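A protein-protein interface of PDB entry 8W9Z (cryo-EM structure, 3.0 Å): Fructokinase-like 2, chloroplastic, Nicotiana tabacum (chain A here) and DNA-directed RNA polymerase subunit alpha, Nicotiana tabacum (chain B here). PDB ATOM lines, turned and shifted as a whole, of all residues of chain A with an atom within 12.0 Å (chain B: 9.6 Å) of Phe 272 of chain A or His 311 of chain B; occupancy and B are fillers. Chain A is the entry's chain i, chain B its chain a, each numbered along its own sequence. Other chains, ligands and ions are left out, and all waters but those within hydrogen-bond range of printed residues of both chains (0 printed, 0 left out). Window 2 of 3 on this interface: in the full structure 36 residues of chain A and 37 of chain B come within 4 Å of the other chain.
The side-chain carboxylate (OD2) of Asp 412 of chain A lies within hydrogen-bond range of the side-chain hydroxyl (OG) of Ser 281 of chain B (2.9 Å). OG of Ser 273 of chain A lies within hydrogen-bond range of SG of Cys 286 of chain B (3.6 Å). The backbone carbonyl oxygen of Ser 273 of chain A sits close to the side-chain amide oxygen of Asn 285 of chain B.
The backbone carbonyl oxygen of Ser 281 of chain B lies within hydrogen-bond range of the side-chain amide nitrogen of Asn 285 of chain B, at 2.5 Å. The guanidinium group (NH2) of Arg 368 of chain A is in salt-bridge range of the side-chain carboxylate (OE1) of Glu 416 of chain A, at 2.8 Å. The side-chain amide oxygen (OD1) of Asn 285 of chain B is in hydrogen-bond range of the side-chain sulfur (SG) of Cys 286 of chain B (3.6 Å). The backbone carbonyl oxygen (O) of Arg 282 of chain B sits close to the side-chain amide oxygen (OD1) of Asn 285 of chain B (2.7 Å). The backbone carbonyl oxygen of Arg 282 of chain B lies within hydrogen-bond range of the side-chain sulfur of Cys 286 of chain B (3.2 Å).
Among the printed residues, pairs that only touch across the chains: Asp 269 of chain A with Arg 282 of chain B (3.2 Å), Arg 368 of chain A with Tyr 284 of chain B (3.3 Å), Phe 272 of chain A with His 311 of chain B (3.4 Å), Ser 273 of chain A with Met 289 of chain B (3.7 Å) and Arg 368 of chain A with Ser 281 of chain B (3.8 Å).
Phe 272 of chain A touches just one residue of chain B: His 311 (3.4 Å). Ser 273 of chain A touches three residues of chain B. Gly 275 of chain A touches none of the printed residues of chain B. Of the printed residues of chain B, Asp 412 of chain A touches Ser 281 (2.9 Å). Of the printed residues of chain A, Arg 282 of chain B touches Asp 269. Cys 286 of chain B touches just one residue of chain A: Ser 273 (3.6 Å). No residue of chain A comes within 4 Å of Ile 309 of chain B. No residue of chain A comes within 4 Å of Phe 312 of chain B.
Of the 19 printed residues of chain B, 7 touch a printed residue of chain A. Hydrophobic or aromatic side chains of chain B that line the printed part of chain A: Tyr 284, Met 289 and His 311. Along chain B the printed residues that touch a printed residue of chain A span positions 281 to 311. Of the 18 printed residues of chain A, 5 touch a printed residue of chain B. Hydrophobic or aromatic side chains of chain A that line the printed part of chain B: Phe 272. Along chain A the printed residues that touch a printed residue of chain B span positions 269 to 412. Among the printed residues, 8 pairs touch across the chains. Among the printed residues, no Asp or Glu carboxylate lies within 4 Å of a Lys or Arg side-chain nitrogen of the other chain.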
ATOM      1  N   ASP A 265      27.907 -27.144 -16.633  1.00  0.00           N
ATOM      2  CA  ASP A 265      27.469 -28.044 -15.572  1.00  0.00           C
ATOM      3  C   ASP A 265      28.612 -28.381 -14.621  1.00  0.00           C
ATOM      4  O   ASP A 265      28.547 -28.077 -13.423  1.00  0.00           O
ATOM      5  CB  ASP A 265      26.869 -29.317 -16.178  1.00  0.00           C
ATOM      6  CG  ASP A 265      27.701 -29.871 -17.319  1.00  0.00           C
ATOM      7  OD1 ASP A 265      28.747 -29.269 -17.641  1.00  0.00           O
ATOM      8  OD2 ASP A 265      27.310 -30.909 -17.892  1.00  0.00           O
ATOM      9  N   GLY A 266      29.672 -28.998 -15.137  1.00  0.00           N
ATOM     10  CA  GLY A 266      30.793 -29.367 -14.291  1.00  0.00           C
ATOM     11  C   GLY A 266      30.389 -30.384 -13.243  1.00  0.00           C
ATOM     12  O   GLY A 266      29.695 -31.368 -13.527  1.00  0.00           O
ATOM     13  N   GLY A 267      30.827 -30.146 -12.009  1.00  0.00           N
ATOM     14  CA  GLY A 267      30.455 -31.018 -10.908  1.00  0.00           C
ATOM     15  C   GLY A 267      29.032 -30.747 -10.444  1.00  0.00           C
ATOM     16  O   GLY A 267      28.573 -29.607 -10.397  1.00  0.00           O
ATOM     17  N   GLU A 268      28.329 -31.823 -10.097  1.00  0.00           N
ATOM     18  CA  GLU A 268      26.934 -31.750  -9.671  1.00  0.00           C
ATOM     19  C   GLU A 268      26.897 -31.681  -8.148  1.00  0.00           C
ATOM     20  O   GLU A 268      27.105 -32.686  -7.463  1.00  0.00           O
ATOM     21  CB  GLU A 268      26.145 -32.944 -10.198  1.00  0.00           C
ATOM     22  CG  GLU A 268      26.132 -33.061 -11.716  1.00  0.00           C
ATOM     23  CD  GLU A 268      25.391 -31.921 -12.390  1.00  0.00           C
ATOM     24  OE1 GLU A 268      24.511 -31.314 -11.742  1.00  0.00           O
ATOM     25  OE2 GLU A 268      25.687 -31.632 -13.567  1.00  0.00           O
ATOM     26  N   ASP A 269      26.631 -30.488  -7.623  1.00  0.00           N
ATOM     27  CA  ASP A 269      26.507 -30.251  -6.189  1.00  0.00           C
ATOM     28  C   ASP A 269      25.079 -29.861  -5.817  1.00  0.00           C
ATOM     29  O   ASP A 269      24.853 -28.994  -4.972  1.00  0.00           O
ATOM     30  CB  ASP A 269      27.491 -29.178  -5.732  1.00  0.00           C
ATOM     31  CG  ASP A 269      27.348 -27.887  -6.514  1.00  0.00           C
ATOM     32  OD1 ASP A 269      26.623 -27.883  -7.531  1.00  0.00           O
ATOM     33  OD2 ASP A 269      27.955 -26.874  -6.108  1.00  0.00           O
ATOM     34  N   ILE A 270      24.098 -30.504  -6.451  1.00  0.00           N
ATOM     35  CA  ILE A 270      22.705 -30.122  -6.244  1.00  0.00           C
ATOM     36  C   ILE A 270      22.208 -30.608  -4.886  1.00  0.00           C
ATOM     37  O   ILE A 270      21.700 -29.824  -4.077  1.00  0.00           O
ATOM     38  CB  ILE A 270      21.829 -30.648  -7.396  1.00  0.00           C
ATOM     39  CG1 ILE A 270      22.236 -32.070  -7.785  1.00  0.00           C
ATOM     40  CG2 ILE A 270      21.921 -29.721  -8.600  1.00  0.00           C
ATOM     41  CD1 ILE A 270      21.429 -32.644  -8.930  1.00  0.00           C
ATOM     42  N   SER A 271      22.355 -31.901  -4.611  1.00  0.00           N
ATOM     43  CA  SER A 271      21.837 -32.493  -3.385  1.00  0.00           C
ATOM     44  C   SER A 271      22.819 -32.411  -2.220  1.00  0.00           C
ATOM     45  O   SER A 271      22.520 -32.935  -1.143  1.00  0.00           O
ATOM     46  CB  SER A 271      21.455 -33.955  -3.627  1.00  0.00           C
ATOM     47  OG  SER A 271      20.526 -34.071  -4.692  1.00  0.00           O
ATOM     48  N   PHE A 272      23.974 -31.775  -2.407  1.00  0.00           N
ATOM     49  CA  PHE A 272      24.988 -31.753  -1.354  1.00  0.00           C
ATOM     50  C   PHE A 272      24.702 -30.675  -0.312  1.00  0.00           C
ATOM     51  O   PHE A 272      24.518 -30.974   0.870  1.00  0.00           O
ATOM     52  CB  PHE A 272      26.379 -31.568  -1.975  1.00  0.00           C
ATOM     53  CG  PHE A 272      26.907 -32.804  -2.641  1.00  0.00           C
ATOM     54  CD1 PHE A 272      26.641 -33.058  -3.976  1.00  0.00           C
ATOM     55  CD2 PHE A 272      27.663 -33.719  -1.928  1.00  0.00           C
ATOM     56  CE1 PHE A 272      27.124 -34.198  -4.589  1.00  0.00           C
ATOM     57  CE2 PHE A 272      28.148 -34.861  -2.535  1.00  0.00           C
ATOM     58  CZ  PHE A 272      27.878 -35.101  -3.867  1.00  0.00           C
ATOM     59  N   SER A 273      24.664 -29.412  -0.732  1.00  0.00           N
ATOM     60  CA  SER A 273      24.490 -28.292   0.188  1.00  0.00           C
ATOM     61  C   SER A 273      23.671 -27.176  -0.453  1.00  0.00           C
ATOM     62  O   SER A 273      24.060 -26.006  -0.446  1.00  0.00           O
ATOM     63  CB  SER A 273      25.842 -27.771   0.662  1.00  0.00           C
ATOM     64  OG  SER A 273      26.649 -27.379  -0.435  1.00  0.00           O
ATOM     65  N   TYR A 274      22.520 -27.523  -1.028  1.00  0.00           N
ATOM     66  CA  TYR A 274      21.622 -26.508  -1.564  1.00  0.00           C
ATOM     67  C   TYR A 274      20.625 -25.986  -0.542  1.00  0.00           C
ATOM     68  O   TYR A 274      20.103 -24.879  -0.718  1.00  0.00           O
ATOM     69  CB  TYR A 274      20.853 -27.049  -2.773  1.00  0.00           C
ATOM     70  CG  TYR A 274      21.516 -26.763  -4.098  1.00  0.00           C
ATOM     71  CD1 TYR A 274      22.769 -26.169  -4.158  1.00  0.00           C
ATOM     72  CD2 TYR A 274      20.882 -27.075  -5.293  1.00  0.00           C
ATOM     73  CE1 TYR A 274      23.376 -25.904  -5.368  1.00  0.00           C
ATOM     74  CE2 TYR A 274      21.481 -26.812  -6.508  1.00  0.00           C
ATOM     75  CZ  TYR A 274      22.728 -26.227  -6.540  1.00  0.00           C
ATOM     76  OH  TYR A 274      23.331 -25.963  -7.748  1.00  0.00           O
ATOM     77  N   GLY A 275      20.339 -26.748   0.510  1.00  0.00           N
ATOM     78  CA  GLY A 275      19.375 -26.326   1.507  1.00  0.00           C
ATOM     79  C   GLY A 275      17.946 -26.398   1.010  1.00  0.00           C
ATOM     80  O   GLY A 275      17.707 -26.485  -0.198  1.00  0.00           O
ATOM     81  N   TRP A 276      16.984 -26.361   1.929  1.00  0.00           N
ATOM     82  CA  TRP A 276      15.589 -26.468   1.517  1.00  0.00           C
ATOM     83  C   TRP A 276      15.094 -25.186   0.850  1.00  0.00           C
ATOM     84  O   TRP A 276      14.637 -25.254  -0.298  1.00  0.00           O
ATOM     85  CB  TRP A 276      14.688 -26.847   2.698  1.00  0.00           C
ATOM     86  CG  TRP A 276      13.271 -26.365   2.549  1.00  0.00           C
ATOM     87  CD1 TRP A 276      12.575 -25.592   3.431  1.00  0.00           C
ATOM     88  CD2 TRP A 276      12.385 -26.612   1.446  1.00  0.00           C
ATOM     89  NE1 TRP A 276      11.311 -25.347   2.952  1.00  0.00           N
ATOM     90  CE2 TRP A 276      11.171 -25.960   1.735  1.00  0.00           C
ATOM     91  CE3 TRP A 276      12.502 -27.318   0.245  1.00  0.00           C
ATOM     92  CZ2 TRP A 276      10.083 -25.996   0.868  1.00  0.00           C
ATOM     93  CZ3 TRP A 276      11.421 -27.351  -0.613  1.00  0.00           C
ATOM     94  CH2 TRP A 276      10.228 -26.696  -0.298  1.00  0.00           C
ATOM     95  N   PRO A 277      15.151 -24.017   1.497  1.00  0.00           N
ATOM     96  CA  PRO A 277      14.566 -22.813   0.888  1.00  0.00           C
ATOM     97  C   PRO A 277      15.191 -22.527  -0.465  1.00  0.00           C
ATOM     98  O   PRO A 277      16.393 -22.238  -0.556  1.00  0.00           O
ATOM     99  CB  PRO A 277      14.893 -21.705   1.899  1.00  0.00           C
ATOM    100  CG  PRO A 277      15.106 -22.413   3.178  1.00  0.00           C
ATOM    101  CD  PRO A 277      15.769 -23.697   2.799  1.00  0.00           C
ATOM    102  N   LYS A 340      15.505 -17.194   1.015  1.00  0.00           N
ATOM    103  CA  LYS A 340      16.887 -17.180   0.550  1.00  0.00           C
ATOM    104  C   LYS A 340      16.933 -16.437  -0.781  1.00  0.00           C
ATOM    105  O   LYS A 340      16.402 -16.919  -1.787  1.00  0.00           O
ATOM    106  CB  LYS A 340      17.428 -18.601   0.415  1.00  0.00           C
ATOM    107  CG  LYS A 340      18.923 -18.677   0.165  1.00  0.00           C
ATOM    108  CD  LYS A 340      19.397 -20.119   0.088  1.00  0.00           C
ATOM    109  CE  LYS A 340      19.142 -20.854   1.393  1.00  0.00           C
ATOM    110  NZ  LYS A 340      19.620 -22.263   1.339  1.00  0.00           N
ATOM    111  N   ARG A 368      26.973 -12.658  -3.728  1.00  0.00           N
ATOM    112  CA  ARG A 368      28.031 -13.313  -4.453  1.00  0.00           C
ATOM    113  C   ARG A 368      27.900 -13.005  -5.921  1.00  0.00           C
ATOM    114  O   ARG A 368      28.886 -12.750  -6.592  1.00  0.00           O
ATOM    115  CB  ARG A 368      27.981 -14.810  -4.228  1.00  0.00           C
ATOM    116  CG  ARG A 368      26.593 -15.407  -4.213  1.00  0.00           C
ATOM    117  CD  ARG A 368      26.640 -16.850  -4.666  1.00  0.00           C
ATOM    118  NE  ARG A 368      25.625 -17.651  -4.002  1.00  0.00           N
ATOM    119  CZ  ARG A 368      25.408 -18.932  -4.259  1.00  0.00           C
ATOM    120  NH1 ARG A 368      26.124 -19.556  -5.180  1.00  0.00           N
ATOM    121  NH2 ARG A 368      24.468 -19.587  -3.599  1.00  0.00           N
ATOM    122  N   ASP A 412      26.324 -20.185 -12.029  1.00  0.00           N
ATOM    123  CA  ASP A 412      26.080 -21.083 -10.919  1.00  0.00           C
ATOM    124  C   ASP A 412      24.875 -20.698 -10.103  1.00  0.00           C
ATOM    125  O   ASP A 412      24.122 -21.558  -9.669  1.00  0.00           O
ATOM    126  CB  ASP A 412      27.299 -21.171 -10.029  1.00  0.00           C
ATOM    127  CG  ASP A 412      27.556 -22.579  -9.544  1.00  0.00           C
ATOM    128  OD1 ASP A 412      26.578 -23.317  -9.306  1.00  0.00           O
ATOM    129  OD2 ASP A 412      28.737 -22.949  -9.399  1.00  0.00           O
ATOM    130  N   LYS A 415      21.759 -21.805 -11.744  1.00  0.00           N
ATOM    131  CA  LYS A 415      21.570 -23.248 -11.643  1.00  0.00           C
ATOM    132  C   LYS A 415      20.938 -23.627 -10.311  1.00  0.00           C
ATOM    133  O   LYS A 415      20.063 -24.499 -10.257  1.00  0.00           O
ATOM    134  CB  LYS A 415      22.907 -23.965 -11.825  1.00  0.00           C
ATOM    135  CG  LYS A 415      22.818 -25.479 -11.750  1.00  0.00           C
ATOM    136  CD  LYS A 415      24.201 -26.111 -11.751  1.00  0.00           C
ATOM    137  CE  LYS A 415      24.994 -25.702 -12.981  1.00  0.00           C
ATOM    138  NZ  LYS A 415      26.377 -26.251 -12.951  1.00  0.00           N
ATOM    139  N   GLU A 416      21.367 -22.981  -9.225  1.00  0.00           N
ATOM    140  CA  GLU A 416      20.797 -23.264  -7.914  1.00  0.00           C
ATOM    141  C   GLU A 416      19.414 -22.648  -7.743  1.00  0.00           C
ATOM    142  O   GLU A 416      18.562 -23.231  -7.064  1.00  0.00           O
ATOM    143  CB  GLU A 416      21.736 -22.759  -6.818  1.00  0.00           C
ATOM    144  CG  GLU A 416      21.236 -22.991  -5.403  1.00  0.00           C
ATOM    145  CD  GLU A 416      22.183 -22.444  -4.354  1.00  0.00           C
ATOM    146  OE1 GLU A 416      23.220 -21.862  -4.734  1.00  0.00           O
ATOM    147  OE2 GLU A 416      21.889 -22.596  -3.150  1.00  0.00           O
ATOM    148  N   SER B 281      31.203 -22.152  -5.324  1.00  0.00           N
ATOM    149  CA  SER B 281      29.854 -22.186  -4.769  1.00  0.00           C
ATOM    150  C   SER B 281      29.729 -23.208  -3.648  1.00  0.00           C
ATOM    151  O   SER B 281      28.984 -22.982  -2.686  1.00  0.00           O
ATOM    152  CB  SER B 281      28.842 -22.479  -5.875  1.00  0.00           C
ATOM    153  OG  SER B 281      28.899 -21.490  -6.887  1.00  0.00           O
ATOM    154  N   ARG B 282      30.448 -24.328  -3.746  1.00  0.00           N
ATOM    155  CA  ARG B 282      30.345 -25.374  -2.734  1.00  0.00           C
ATOM    156  C   ARG B 282      30.801 -24.867  -1.371  1.00  0.00           C
ATOM    157  O   ARG B 282      30.067 -24.957  -0.380  1.00  0.00           O
ATOM    158  CB  ARG B 282      31.165 -26.594  -3.157  1.00  0.00           C
ATOM    159  CG  ARG B 282      30.719 -27.227  -4.462  1.00  0.00           C
ATOM    160  CD  ARG B 282      31.563 -28.446  -4.797  1.00  0.00           C
ATOM    161  NE  ARG B 282      31.488 -29.465  -3.753  1.00  0.00           N
ATOM    162  CZ  ARG B 282      32.122 -30.632  -3.802  1.00  0.00           C
ATOM    163  NH1 ARG B 282      32.883 -30.933  -4.846  1.00  0.00           N
ATOM    164  NH2 ARG B 282      31.997 -31.499  -2.807  1.00  0.00           N
ATOM    165  N   ILE B 283      32.025 -24.337  -1.304  1.00  0.00           N
ATOM    166  CA  ILE B 283      32.550 -23.833  -0.039  1.00  0.00           C
ATOM    167  C   ILE B 283      31.686 -22.691   0.478  1.00  0.00           C
ATOM    168  O   ILE B 283      31.427 -22.582   1.683  1.00  0.00           O
ATOM    169  CB  ILE B 283      34.021 -23.406  -0.200  1.00  0.00           C
ATOM    170  CG1 ILE B 283      34.901 -24.608  -0.556  1.00  0.00           C
ATOM    171  CG2 ILE B 283      34.532 -22.737   1.068  1.00  0.00           C
ATOM    172  CD1 ILE B 283      35.105 -24.815  -2.045  1.00  0.00           C
ATOM    173  N   TYR B 284      31.207 -21.835  -0.427  1.00  0.00           N
ATOM    174  CA  TYR B 284      30.386 -20.698  -0.025  1.00  0.00           C
ATOM    175  C   TYR B 284      29.103 -21.158   0.656  1.00  0.00           C
ATOM    176  O   TYR B 284      28.789 -20.732   1.773  1.00  0.00           O
ATOM    177  CB  TYR B 284      30.069 -19.824  -1.239  1.00  0.00           C
ATOM    178  CG  TYR B 284      29.131 -18.682  -0.930  1.00  0.00           C
ATOM    179  CD1 TYR B 284      29.598 -17.514  -0.345  1.00  0.00           C
ATOM    180  CD2 TYR B 284      27.777 -18.772  -1.223  1.00  0.00           C
ATOM    181  CE1 TYR B 284      28.744 -16.468  -0.060  1.00  0.00           C
ATOM    182  CE2 TYR B 284      26.916 -17.731  -0.939  1.00  0.00           C
ATOM    183  CZ  TYR B 284      27.405 -16.582  -0.361  1.00  0.00           C
ATOM    184  OH  TYR B 284      26.551 -15.542  -0.078  1.00  0.00           O
ATOM    185  N   ASN B 285      28.339 -22.029  -0.008  1.00  0.00           N
ATOM    186  CA  ASN B 285      27.080 -22.468   0.581  1.00  0.00           C
ATOM    187  C   ASN B 285      27.292 -23.362   1.795  1.00  0.00           C
ATOM    188  O   ASN B 285      26.440 -23.376   2.691  1.00  0.00           O
ATOM    189  CB  ASN B 285      26.212 -23.171  -0.469  1.00  0.00           C
ATOM    190  CG  ASN B 285      26.889 -24.377  -1.087  1.00  0.00           C
ATOM    191  OD1 ASN B 285      27.391 -25.254  -0.388  1.00  0.00           O
ATOM    192  ND2 ASN B 285      26.903 -24.427  -2.414  1.00  0.00           N
ATOM    193  N   CYS B 286      28.415 -24.084   1.868  1.00  0.00           N
ATOM    194  CA  CYS B 286      28.694 -24.867   3.066  1.00  0.00           C
ATOM    195  C   CYS B 286      28.988 -23.964   4.257  1.00  0.00           C
ATOM    196  O   CYS B 286      28.506 -24.217   5.367  1.00  0.00           O
ATOM    197  CB  CYS B 286      29.858 -25.824   2.814  1.00  0.00           C
ATOM    198  SG  CYS B 286      29.454 -27.223   1.742  1.00  0.00           S
ATOM    199  N   LEU B 287      29.769 -22.902   4.047  1.00  0.00           N
ATOM    200  CA  LEU B 287      30.009 -21.948   5.124  1.00  0.00           C
ATOM    201  C   LEU B 287      28.740 -21.189   5.489  1.00  0.00           C
ATOM    202  O   LEU B 287      28.563 -20.805   6.651  1.00  0.00           O
ATOM    203  CB  LEU B 287      31.118 -20.973   4.730  1.00  0.00           C
ATOM    204  CG  LEU B 287      32.521 -21.564   4.587  1.00  0.00           C
ATOM    205  CD1 LEU B 287      33.522 -20.485   4.206  1.00  0.00           C
ATOM    206  CD2 LEU B 287      32.941 -22.262   5.871  1.00  0.00           C
ATOM    207  N   MET B 289      25.671 -22.507   5.368  1.00  0.00           N
ATOM    208  CA  MET B 289      24.890 -23.436   6.177  1.00  0.00           C
ATOM    209  C   MET B 289      25.497 -23.650   7.557  1.00  0.00           C
ATOM    210  O   MET B 289      24.805 -24.143   8.454  1.00  0.00           O
ATOM    211  CB  MET B 289      24.750 -24.778   5.458  1.00  0.00           C
ATOM    212  CG  MET B 289      23.894 -24.723   4.204  1.00  0.00           C
ATOM    213  SD  MET B 289      23.743 -26.328   3.397  1.00  0.00           S
ATOM    214  CE  MET B 289      22.995 -27.295   4.704  1.00  0.00           C
ATOM    215  N   LEU B 306      36.841 -26.465  10.695  1.00  0.00           N
ATOM    216  CA  LEU B 306      36.385 -26.595   9.317  1.00  0.00           C
ATOM    217  C   LEU B 306      36.242 -28.045   8.872  1.00  0.00           C
ATOM    218  O   LEU B 306      35.820 -28.284   7.736  1.00  0.00           O
ATOM    219  CB  LEU B 306      37.338 -25.863   8.367  1.00  0.00           C
ATOM    220  CG  LEU B 306      37.134 -24.358   8.165  1.00  0.00           C
ATOM    221  CD1 LEU B 306      37.516 -23.564   9.405  1.00  0.00           C
ATOM    222  CD2 LEU B 306      37.918 -23.872   6.953  1.00  0.00           C
ATOM    223  N   MET B 307      36.586 -29.010   9.722  1.00  0.00           N
ATOM    224  CA  MET B 307      36.464 -30.419   9.377  1.00  0.00           C
ATOM    225  C   MET B 307      35.198 -31.064   9.922  1.00  0.00           C
ATOM    226  O   MET B 307      34.702 -32.027   9.326  1.00  0.00           O
ATOM    227  CB  MET B 307      37.685 -31.196   9.886  1.00  0.00           C
ATOM    228  CG  MET B 307      37.836 -32.585   9.286  1.00  0.00           C
ATOM    229  SD  MET B 307      38.009 -32.545   7.491  1.00  0.00           S
ATOM    230  CE  MET B 307      38.154 -34.292   7.124  1.00  0.00           C
ATOM    231  N   LYS B 308      34.658 -30.556  11.033  1.00  0.00           N
ATOM    232  CA  LYS B 308      33.446 -31.140  11.599  1.00  0.00           C
ATOM    233  C   LYS B 308      32.238 -30.927  10.696  1.00  0.00           C
ATOM    234  O   LYS B 308      31.303 -31.735  10.717  1.00  0.00           O
ATOM    235  CB  LYS B 308      33.174 -30.561  12.988  1.00  0.00           C
ATOM    236  CG  LYS B 308      33.678 -31.424  14.135  1.00  0.00           C
ATOM    237  CD  LYS B 308      35.193 -31.410  14.230  1.00  0.00           C
ATOM    238  CE  LYS B 308      35.701 -30.049  14.675  1.00  0.00           C
ATOM    239  NZ  LYS B 308      37.184 -30.032  14.814  1.00  0.00           N
ATOM    240  N   ILE B 309      32.232 -29.852   9.907  1.00  0.00           N
ATOM    241  CA  ILE B 309      31.126 -29.603   8.992  1.00  0.00           C
ATOM    242  C   ILE B 309      31.134 -30.649   7.885  1.00  0.00           C
ATOM    243  O   ILE B 309      32.184 -30.964   7.307  1.00  0.00           O
ATOM    244  CB  ILE B 309      31.209 -28.176   8.424  1.00  0.00           C
ATOM    245  CG1 ILE B 309      30.199 -27.985   7.290  1.00  0.00           C
ATOM    246  CG2 ILE B 309      32.621 -27.864   7.956  1.00  0.00           C
ATOM    247  CD1 ILE B 309      30.253 -26.618   6.653  1.00  0.00           C
ATOM    248  N   GLU B 310      29.959 -31.199   7.590  1.00  0.00           N
ATOM    249  CA  GLU B 310      29.852 -32.259   6.601  1.00  0.00           C
ATOM    250  C   GLU B 310      30.080 -31.711   5.194  1.00  0.00           C
ATOM    251  O   GLU B 310      30.078 -30.499   4.956  1.00  0.00           O
ATOM    252  CB  GLU B 310      28.484 -32.936   6.692  1.00  0.00           C
ATOM    253  N   HIS B 311      30.285 -32.636   4.254  1.00  0.00           N
ATOM    254  CA  HIS B 311      30.471 -32.312   2.838  1.00  0.00           C
ATOM    255  C   HIS B 311      31.673 -31.393   2.625  1.00  0.00           C
ATOM    256  O   HIS B 311      31.635 -30.472   1.808  1.00  0.00           O
ATOM    257  CB  HIS B 311      29.203 -31.699   2.240  1.00  0.00           C
ATOM    258  CG  HIS B 311      27.989 -32.564   2.380  1.00  0.00           C
ATOM    259  ND1 HIS B 311      27.611 -33.476   1.418  1.00  0.00           N
ATOM    260  CD2 HIS B 311      27.070 -32.657   3.371  1.00  0.00           C
ATOM    261  CE1 HIS B 311      26.509 -34.092   1.810  1.00  0.00           C
ATOM    262  NE2 HIS B 311      26.162 -33.614   2.991  1.00  0.00           N
ATOM    263  N   PHE B 312      32.750 -31.646   3.365  1.00  0.00           N
ATOM    264  CA  PHE B 312      33.982 -30.885   3.226  1.00  0.00           C
ATOM    265  C   PHE B 312      35.159 -31.835   3.050  1.00  0.00           C
ATOM    266  O   PHE B 312      35.086 -33.021   3.381  1.00  0.00           O
ATOM    267  CB  PHE B 312      34.225 -29.966   4.431  1.00  0.00           C
ATOM    268  N   ARG B 313      36.252 -31.290   2.518  1.00  0.00           N
ATOM    269  CA  ARG B 313      37.453 -32.068   2.239  1.00  0.00           C
ATOM    270  C   ARG B 313      38.681 -31.387   2.831  1.00  0.00           C
ATOM    271  O   ARG B 313      38.557 -30.461   3.639  1.00  0.00           O
ATOM    272  CB  ARG B 313      37.626 -32.266   0.732  1.00  0.00           C
ATOM    273  CG  ARG B 313      37.844 -30.978  -0.043  1.00  0.00           C
ATOM    274  CD  ARG B 313      37.930 -31.225  -1.543  1.00  0.00           C
ATOM    275  NE  ARG B 313      36.649 -31.642  -2.110  1.00  0.00           N
ATOM    276  CZ  ARG B 313      36.326 -32.901  -2.387  1.00  0.00           C
ATOM    277  NH1 ARG B 313      37.190 -33.878  -2.152  1.00  0.00           N
ATOM    278  NH2 ARG B 313      35.136 -33.184  -2.902  1.00  0.00           N
ATOM    279  N   SER B 314      39.872 -31.855   2.455  1.00  0.00           N
ATOM    280  CA  SER B 314      41.114 -31.242   2.904  1.00  0.00           C
ATOM    281  C   SER B 314      41.696 -30.254   1.903  1.00  0.00           C
ATOM    282  O   SER B 314      42.534 -29.432   2.287  1.00  0.00           O
ATOM    283  CB  SER B 314      42.160 -32.323   3.207  1.00  0.00           C
ATOM    284  OG  SER B 314      41.709 -33.198   4.226  1.00  0.00           O
ATOM    285  N   ASP B 316      39.891 -27.965  -0.015  1.00  0.00           N
ATOM    286  CA  ASP B 316      39.230 -26.668   0.084  1.00  0.00           C
ATOM    287  C   ASP B 316      39.777 -25.849   1.245  1.00  0.00           C
ATOM    288  O   ASP B 316      39.743 -24.615   1.204  1.00  0.00           O
ATOM    289  CB  ASP B 316      37.719 -26.857   0.221  1.00  0.00           C
ATOM    290  CG  ASP B 316      37.348 -27.804   1.342  1.00  0.00           C
ATOM    291  OD1 ASP B 316      38.256 -28.251   2.072  1.00  0.00           O
ATOM    292  OD2 ASP B 316      36.147 -28.107   1.490  1.00  0.00           O
ATOM    293  N   VAL B 317      40.287 -26.514   2.286  1.00  0.00           N
ATOM    294  CA  VAL B 317      40.962 -25.794   3.362  1.00  0.00           C
ATOM    295  C   VAL B 317      42.211 -25.104   2.828  1.00  0.00           C
ATOM    296  O   VAL B 317      42.479 -23.938   3.141  1.00  0.00           O
ATOM    297  CB  VAL B 317      41.293 -26.751   4.521  1.00  0.00           C
ATOM    298  CG1 VAL B 317      41.960 -25.995   5.659  1.00  0.00           C
ATOM    299  CG2 VAL B 317      40.033 -27.452   5.003  1.00  0.00           C
